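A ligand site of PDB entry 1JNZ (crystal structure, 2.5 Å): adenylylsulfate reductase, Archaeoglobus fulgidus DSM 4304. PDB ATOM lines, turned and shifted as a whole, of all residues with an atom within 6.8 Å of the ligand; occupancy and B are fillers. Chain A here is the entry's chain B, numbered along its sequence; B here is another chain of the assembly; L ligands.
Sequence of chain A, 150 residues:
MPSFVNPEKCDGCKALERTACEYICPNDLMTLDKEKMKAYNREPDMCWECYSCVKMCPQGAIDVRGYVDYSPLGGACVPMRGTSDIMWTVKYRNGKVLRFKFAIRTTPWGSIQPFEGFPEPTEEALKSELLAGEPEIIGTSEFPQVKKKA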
ATOM      1  N   PRO A   2      21.045  31.556  14.568  1.00  0.00           N
ATOM      2  CA  PRO A   2      21.763  30.923  15.693  1.00  0.00           C
ATOM      3  C   PRO A   2      21.544  29.419  15.736  1.00  0.00           C
ATOM      4  O   PRO A   2      20.596  28.892  15.151  1.00  0.00           O
ATOM      5  CB  PRO A   2      21.248  31.568  16.967  1.00  0.00           C
ATOM      6  CG  PRO A   2      20.820  32.929  16.460  1.00  0.00           C
ATOM      7  CD  PRO A   2      20.206  32.652  15.072  1.00  0.00           C
ATOM      8  N   SER A   3      22.430  28.720  16.435  1.00  0.00           N
ATOM      9  CA  SER A   3      22.325  27.271  16.545  1.00  0.00           C
ATOM     10  C   SER A   3      21.308  26.883  17.607  1.00  0.00           C
ATOM     11  O   SER A   3      20.946  27.694  18.467  1.00  0.00           O
ATOM     12  CB  SER A   3      23.680  26.668  16.907  1.00  0.00           C
ATOM     13  OG  SER A   3      24.141  27.204  18.130  1.00  0.00           O
ATOM     14  N   CYS A  21      30.018  19.937  21.253  1.00  0.00           N
ATOM     15  CA  CYS A  21      29.543  21.302  21.024  1.00  0.00           C
ATOM     16  C   CYS A  21      30.160  22.317  21.988  1.00  0.00           C
ATOM     17  O   CYS A  21      30.590  23.389  21.566  1.00  0.00           O
ATOM     18  CB  CYS A  21      28.021  21.353  21.119  1.00  0.00           C
ATOM     19  SG  CYS A  21      27.335  20.933  22.740  1.00  0.00           S
ATOM     20  N   ILE A  24      33.983  22.844  21.092  1.00  0.00           N
ATOM     21  CA  ILE A  24      34.322  23.551  19.860  1.00  0.00           C
ATOM     22  C   ILE A  24      33.943  25.028  19.679  1.00  0.00           C
ATOM     23  O   ILE A  24      34.678  25.779  19.040  1.00  0.00           O
ATOM     24  CB  ILE A  24      33.780  22.766  18.643  1.00  0.00           C
ATOM     25  CG1 ILE A  24      34.613  23.090  17.389  1.00  0.00           C
ATOM     26  CG2 ILE A  24      32.321  23.096  18.400  1.00  0.00           C
ATOM     27  CD1 ILE A  24      36.058  22.633  17.474  1.00  0.00           C
ATOM     28  N   CYS A  25      32.810  25.450  20.231  1.00  0.00           N
ATOM     29  CA  CYS A  25      32.341  26.828  20.073  1.00  0.00           C
ATOM     30  C   CYS A  25      33.348  27.935  20.378  1.00  0.00           C
ATOM     31  O   CYS A  25      33.761  28.132  21.525  1.00  0.00           O
ATOM     32  CB  CYS A  25      31.078  27.079  20.897  1.00  0.00           C
ATOM     33  SG  CYS A  25      30.473  28.782  20.730  1.00  0.00           S
ATOM     34  N   PRO A  26      33.727  28.710  19.336  1.00  0.00           N
ATOM     35  CA  PRO A  26      34.683  29.827  19.396  1.00  0.00           C
ATOM     36  C   PRO A  26      34.213  30.991  20.253  1.00  0.00           C
ATOM     37  O   PRO A  26      35.010  31.871  20.583  1.00  0.00           O
ATOM     38  CB  PRO A  26      34.821  30.232  17.933  1.00  0.00           C
ATOM     39  CG  PRO A  26      34.468  28.979  17.165  1.00  0.00           C
ATOM     40  CD  PRO A  26      33.291  28.477  17.949  1.00  0.00           C
ATOM     41  N   ASN A  27      32.933  31.008  20.612  1.00  0.00           N
ATOM     42  CA  ASN A  27      32.400  32.102  21.428  1.00  0.00           C
ATOM     43  C   ASN A  27      31.810  31.635  22.754  1.00  0.00           C
ATOM     44  O   ASN A  27      31.087  32.381  23.422  1.00  0.00           O
ATOM     45  CB  ASN A  27      31.362  32.904  20.639  1.00  0.00           C
ATOM     46  CG  ASN A  27      31.451  34.414  20.913  1.00  0.00           C
ATOM     47  OD1 ASN A  27      32.509  34.918  21.303  1.00  0.00           O
ATOM     48  ND2 ASN A  27      30.353  35.126  20.691  1.00  0.00           N
ATOM     49  N   ASP A  28      32.122  30.396  23.141  1.00  0.00           N
ATOM     50  CA  ASP A  28      31.656  29.828  24.395  1.00  0.00           C
ATOM     51  C   ASP A  28      30.140  29.884  24.581  1.00  0.00           C
ATOM     52  O   ASP A  28      29.649  30.207  25.656  1.00  0.00           O
ATOM     53  CB  ASP A  28      32.348  30.563  25.555  1.00  0.00           C
ATOM     54  CG  ASP A  28      32.100  29.903  26.898  1.00  0.00           C
ATOM     55  OD1 ASP A  28      32.262  28.665  26.980  1.00  0.00           O
ATOM     56  OD2 ASP A  28      31.758  30.618  27.868  1.00  0.00           O
ATOM     57  N   LEU A  29      29.401  29.552  23.523  1.00  0.00           N
ATOM     58  CA  LEU A  29      27.940  29.600  23.587  1.00  0.00           C
ATOM     59  C   LEU A  29      27.272  28.288  23.971  1.00  0.00           C
ATOM     60  O   LEU A  29      26.277  28.287  24.693  1.00  0.00           O
ATOM     61  CB  LEU A  29      27.375  30.073  22.254  1.00  0.00           C
ATOM     62  CG  LEU A  29      27.877  31.412  21.714  1.00  0.00           C
ATOM     63  CD1 LEU A  29      27.062  31.794  20.489  1.00  0.00           C
ATOM     64  CD2 LEU A  29      27.786  32.482  22.794  1.00  0.00           C
ATOM     65  N   MET A  30      27.817  27.173  23.494  1.00  0.00           N
ATOM     66  CA  MET A  30      27.249  25.862  23.790  1.00  0.00           C
ATOM     67  C   MET A  30      27.628  25.383  25.187  1.00  0.00           C
ATOM     68  O   MET A  30      28.787  25.402  25.577  1.00  0.00           O
ATOM     69  CB  MET A  30      27.704  24.858  22.745  1.00  0.00           C
ATOM     70  CG  MET A  30      27.351  25.249  21.324  1.00  0.00           C
ATOM     71  SD  MET A  30      25.578  25.602  21.116  1.00  0.00           S
ATOM     72  CE  MET A  30      24.894  23.964  21.347  1.00  0.00           C
ATOM     73  N   ASN A  41      22.345  26.632  23.306  1.00  0.00           N
ATOM     74  CA  ASN A  41      23.099  27.853  23.093  1.00  0.00           C
ATOM     75  C   ASN A  41      22.697  28.812  24.205  1.00  0.00           C
ATOM     76  O   ASN A  41      21.535  29.209  24.312  1.00  0.00           O
ATOM     77  CB  ASN A  41      22.731  28.439  21.733  1.00  0.00           C
ATOM     78  CG  ASN A  41      23.568  29.644  21.381  1.00  0.00           C
ATOM     79  OD1 ASN A  41      23.796  30.521  22.217  1.00  0.00           O
ATOM     80  ND2 ASN A  41      24.025  29.707  20.124  1.00  0.00           N
ATOM     81  N   PRO A  44      22.380  33.087  22.159  1.00  0.00           N
ATOM     82  CA  PRO A  44      22.154  33.126  20.704  1.00  0.00           C
ATOM     83  C   PRO A  44      22.460  34.405  19.930  1.00  0.00           C
ATOM     84  O   PRO A  44      22.877  34.347  18.772  1.00  0.00           O
ATOM     85  CB  PRO A  44      20.699  32.682  20.566  1.00  0.00           C
ATOM     86  CG  PRO A  44      20.081  33.143  21.862  1.00  0.00           C
ATOM     87  CD  PRO A  44      21.132  32.754  22.864  1.00  0.00           C
ATOM     88  N   MET A  46      24.842  36.143  20.210  1.00  0.00           N
ATOM     89  CA  MET A  46      26.294  36.244  20.150  1.00  0.00           C
ATOM     90  C   MET A  46      26.810  35.140  19.235  1.00  0.00           C
ATOM     91  O   MET A  46      28.015  34.893  19.144  1.00  0.00           O
ATOM     92  CB  MET A  46      26.914  36.100  21.551  1.00  0.00           C
ATOM     93  CG  MET A  46      26.911  37.374  22.383  1.00  0.00           C
ATOM     94  SD  MET A  46      27.821  38.724  21.607  1.00  0.00           S
ATOM     95  CE  MET A  46      29.499  38.235  21.957  1.00  0.00           C
ATOM     96  N   CYS A  47      25.877  34.463  18.561  1.00  0.00           N
ATOM     97  CA  CYS A  47      26.201  33.385  17.641  1.00  0.00           C
ATOM     98  C   CYS A  47      26.620  33.952  16.289  1.00  0.00           C
ATOM     99  O   CYS A  47      25.959  34.829  15.733  1.00  0.00           O
ATOM    100  CB  CYS A  47      24.993  32.459  17.483  1.00  0.00           C
ATOM    101  SG  CYS A  47      25.269  31.013  16.416  1.00  0.00           S
ATOM    102  N   TRP A  48      27.731  33.448  15.751  1.00  0.00           N
ATOM    103  CA  TRP A  48      28.267  33.901  14.470  1.00  0.00           C
ATOM    104  C   TRP A  48      27.746  32.992  13.362  1.00  0.00           C
ATOM    105  O   TRP A  48      27.942  33.261  12.177  1.00  0.00           O
ATOM    106  CB  TRP A  48      29.800  33.831  14.516  1.00  0.00           C
ATOM    107  CG  TRP A  48      30.493  34.780  13.578  1.00  0.00           C
ATOM    108  CD1 TRP A  48      30.216  36.103  13.397  1.00  0.00           C
ATOM    109  CD2 TRP A  48      31.643  34.495  12.766  1.00  0.00           C
ATOM    110  NE1 TRP A  48      31.114  36.663  12.520  1.00  0.00           N
ATOM    111  CE2 TRP A  48      31.997  35.701  12.116  1.00  0.00           C
ATOM    112  CE3 TRP A  48      32.405  33.338  12.526  1.00  0.00           C
ATOM    113  CZ2 TRP A  48      33.082  35.787  11.243  1.00  0.00           C
ATOM    114  CZ3 TRP A  48      33.493  33.432  11.660  1.00  0.00           C
ATOM    115  CH2 TRP A  48      33.819  34.645  11.026  1.00  0.00           C
ATOM    116  N   GLU A  49      27.055  31.921  13.767  1.00  0.00           N
ATOM    117  CA  GLU A  49      26.518  30.927  12.829  1.00  0.00           C
ATOM    118  C   GLU A  49      27.678  30.352  12.003  1.00  0.00           C
ATOM    119  O   GLU A  49      27.593  30.261  10.780  1.00  0.00           O
ATOM    120  CB  GLU A  49      25.458  31.531  11.895  1.00  0.00           C
ATOM    121  CG  GLU A  49      24.136  31.888  12.581  1.00  0.00           C
ATOM    122  CD  GLU A  49      22.976  32.108  11.616  1.00  0.00           C
ATOM    123  OE1 GLU A  49      23.197  32.429  10.431  1.00  0.00           O
ATOM    124  OE2 GLU A  49      21.813  31.973  12.052  1.00  0.00           O
ATOM    125  N   CYS A  50      28.745  29.962  12.693  1.00  0.00           N
ATOM    126  CA  CYS A  50      29.918  29.404  12.030  1.00  0.00           C
ATOM    127  C   CYS A  50      29.770  27.904  11.780  1.00  0.00           C
ATOM    128  O   CYS A  50      30.594  27.299  11.089  1.00  0.00           O
ATOM    129  CB  CYS A  50      31.174  29.650  12.881  1.00  0.00           C
ATOM    130  SG  CYS A  50      31.300  28.668  14.392  1.00  0.00           S
ATOM    131  N   TYR A  51      28.722  27.309  12.344  1.00  0.00           N
ATOM    132  CA  TYR A  51      28.415  25.898  12.174  1.00  0.00           C
ATOM    133  C   TYR A  51      29.442  24.909  12.747  1.00  0.00           C
ATOM    134  O   TYR A  51      29.398  23.711  12.435  1.00  0.00           O
ATOM    135  CB  TYR A  51      28.178  25.572  10.698  1.00  0.00           C
ATOM    136  CG  TYR A  51      26.805  25.953  10.198  1.00  0.00           C
ATOM    137  CD1 TYR A  51      26.421  27.292  10.078  1.00  0.00           C
ATOM    138  CD2 TYR A  51      25.875  24.971   9.878  1.00  0.00           C
ATOM    139  CE1 TYR A  51      25.133  27.633   9.630  1.00  0.00           C
ATOM    140  CE2 TYR A  51      24.603  25.293   9.429  1.00  0.00           C
ATOM    141  CZ  TYR A  51      24.236  26.619   9.315  1.00  0.00           C
ATOM    142  OH  TYR A  51      22.973  26.939   8.866  1.00  0.00           O
ATOM    143  N   SER A  52      30.349  25.394  13.582  1.00  0.00           N
ATOM    144  CA  SER A  52      31.359  24.528  14.173  1.00  0.00           C
ATOM    145  C   SER A  52      30.715  23.440  15.014  1.00  0.00           C
ATOM    146  O   SER A  52      31.037  22.254  14.885  1.00  0.00           O
ATOM    147  CB  SER A  52      32.329  25.340  15.032  1.00  0.00           C
ATOM    148  OG  SER A  52      33.125  26.186  14.229  1.00  0.00           O
ATOM    149  N   CYS A  53      29.776  23.834  15.869  1.00  0.00           N
ATOM    150  CA  CYS A  53      29.079  22.886  16.736  1.00  0.00           C
ATOM    151  C   CYS A  53      28.270  21.910  15.881  1.00  0.00           C
ATOM    152  O   CYS A  53      28.323  20.703  16.109  1.00  0.00           O
ATOM    153  CB  CYS A  53      28.149  23.622  17.704  1.00  0.00           C
ATOM    154  SG  CYS A  53      26.894  24.685  16.922  1.00  0.00           S
ATOM    155  N   VAL A  54      27.550  22.432  14.903  1.00  0.00           N
ATOM    156  CA  VAL A  54      26.746  21.587  14.035  1.00  0.00           C
ATOM    157  C   VAL A  54      27.597  20.474  13.418  1.00  0.00           C
ATOM    158  O   VAL A  54      27.211  19.305  13.411  1.00  0.00           O
ATOM    159  CB  VAL A  54      26.090  22.401  12.890  1.00  0.00           C
ATOM    160  CG1 VAL A  54      25.374  21.473  11.932  1.00  0.00           C
ATOM    161  CG2 VAL A  54      25.121  23.430  13.469  1.00  0.00           C
ATOM    162  N   ILE A  62      22.444  19.179  16.323  1.00  0.00           N
ATOM    163  CA  ILE A  62      22.458  20.624  16.259  1.00  0.00           C
ATOM    164  C   ILE A  62      22.195  21.115  14.829  1.00  0.00           C
ATOM    165  O   ILE A  62      22.706  20.550  13.861  1.00  0.00           O
ATOM    166  CB  ILE A  62      23.816  21.182  16.743  1.00  0.00           C
ATOM    167  CG1 ILE A  62      24.155  20.567  18.111  1.00  0.00           C
ATOM    168  CG2 ILE A  62      23.754  22.699  16.861  1.00  0.00           C
ATOM    169  CD1 ILE A  62      25.460  21.065  18.709  1.00  0.00           C
ATOM    170  N   VAL A  64      20.905  25.008  12.561  1.00  0.00           N
ATOM    171  CA  VAL A  64      20.936  26.454  12.645  1.00  0.00           C
ATOM    172  C   VAL A  64      19.662  27.050  12.067  1.00  0.00           C
ATOM    173  O   VAL A  64      19.227  26.697  10.975  1.00  0.00           O
ATOM    174  CB  VAL A  64      22.169  27.035  11.911  1.00  0.00           C
ATOM    175  CG1 VAL A  64      22.113  28.558  11.908  1.00  0.00           C
ATOM    176  CG2 VAL A  64      23.454  26.567  12.604  1.00  0.00           C
ATOM    177  N   ALA B  67      37.033  30.237  11.765  1.00  0.00           N
ATOM    178  CA  ALA B  67      36.188  29.187  12.325  1.00  0.00           C
ATOM    179  C   ALA B  67      35.351  28.433  11.298  1.00  0.00           C
ATOM    180  O   ALA B  67      35.198  27.219  11.401  1.00  0.00           O
ATOM    181  CB  ALA B  67      35.264  29.781  13.395  1.00  0.00           C
ATOM    182  N   ILE B 237      33.433  37.883  15.411  1.00  0.00           N
ATOM    183  CA  ILE B 237      32.757  38.376  16.597  1.00  0.00           C
ATOM    184  C   ILE B 237      33.545  37.936  17.843  1.00  0.00           C
ATOM    185  O   ILE B 237      33.362  38.458  18.944  1.00  0.00           O
ATOM    186  CB  ILE B 237      31.325  37.799  16.660  1.00  0.00           C
ATOM    187  CG1 ILE B 237      30.521  38.476  17.770  1.00  0.00           C
ATOM    188  CG2 ILE B 237      31.389  36.300  16.904  1.00  0.00           C
ATOM    189  CD1 ILE B 237      29.091  37.971  17.878  1.00  0.00           C
ATOM    190  N   PHE B 238      34.433  36.956  17.651  1.00  0.00           N
ATOM    191  CA  PHE B 238      35.239  36.423  18.738  1.00  0.00           C
ATOM    192  C   PHE B 238      36.379  37.360  19.133  1.00  0.00           C
ATOM    193  O   PHE B 238      36.868  37.315  20.258  1.00  0.00           O
ATOM    194  CB  PHE B 238      35.833  35.066  18.346  1.00  0.00           C
ATOM    195  CG  PHE B 238      34.892  34.201  17.541  1.00  0.00           C
ATOM    196  CD1 PHE B 238      35.193  33.875  16.219  1.00  0.00           C
ATOM    197  CD2 PHE B 238      33.695  33.744  18.093  1.00  0.00           C
ATOM    198  CE1 PHE B 238      34.327  33.084  15.462  1.00  0.00           C
ATOM    199  CE2 PHE B 238      32.820  32.955  17.336  1.00  0.00           C
ATOM    200  CZ  PHE B 238      33.143  32.630  16.020  1.00  0.00           C
HETATM  201 FE1  LIG L   1      29.292  28.613  18.604  1.00  0.00          FE
HETATM  202 FE2  LIG L   1      27.168  29.577  17.021  1.00  0.00          FE
HETATM  203 FE3  LIG L   1      29.468  28.694  15.957  1.00  0.00          FE
HETATM  204 FE4  LIG L   1      27.748  26.984  17.172  1.00  0.00          FE
HETATM  205  S1  LIG L   1      27.295  28.245  15.220  1.00  0.00           S
HETATM  206  S2  LIG L   1      29.892  27.012  17.201  1.00  0.00           S
HETATM  207  S3  LIG L   1      27.025  28.258  18.807  1.00  0.00           S
HETATM  208  S4  LIG L   1      29.325  30.504  17.189  1.00  0.00           S
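SG of Cys 50 sits close to OG of Ser 52, at 3.1 Å. The side-chain hydroxyl (OG) of Ser 3 is in hydrogen-bond range of the side-chain sulfur (SD) of Met 30. OE2 of Glu 49 sits close to N of Pro 2 (2.7 Å). N of Asp 28 lies close to SG of Cys 25 (3.3 Å). The backbone NH of Leu 29 sits close to the side-chain sulfur of Cys 25. The backbone NH (N) of Ser 3 lies close to the side-chain sulfur (SG) of Cys 47 (3.6 Å). SG of Cys 25 lies close to N of Asn 27. The backbone NH of Glu 49 lies close to the side-chain sulfur of Cys 47, 3.3 Å away.
Merely in contact with the ligand: Pro 26, Leu 29, Met 30, Glu 49 and Ser 52. Hydrophobic or aromatic side chains that line the ligand: Pro 26, Leu 29 and Met 30. 13 residues have an atom within 4 Å of the ligand: Ser 3, Cys 25, Pro 26, Leu 29, Met 30, Asn 41, Cys 47, Trp 48, Glu 49, Cys 50, Tyr 51, Ser 52 and Cys 53.
An iron atom (FE2) of the ligand is bound by the side-chain sulfur (SG) of Cys 47, 2.5 Å away. OG of Ser 3 lies close to S3 of the ligand, 3.1 Å away. The backbone NH (N) of Tyr 51 lies close to a sulfur (S1) of the ligand, at 3.3 Å. The side-chain amide nitrogen of Asn 41 sits close to a sulfur (S3) of the ligand (3.6 Å). A sulfur (S2) of the ligand sits close to the backbone NH (N) of Cys 53, 3.4 Å away. An iron atom (FE1) of the ligand is bound by the side-chain sulfur (SG) of Cys 25 (2.4 Å). An iron atom (FE3) of the ligand is bound by the side-chain sulfur (SG) of Cys 50, 2.4 Å away. A sulfur (S1) of the ligand sits close to the backbone NH (N) of Cys 50 (3.4 Å). The side-chain sulfur of Cys 53 is bound to an iron atom (FE4) of the ligand. S4 of the ligand lies close to N of Trp 48, at 3.6 Å.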
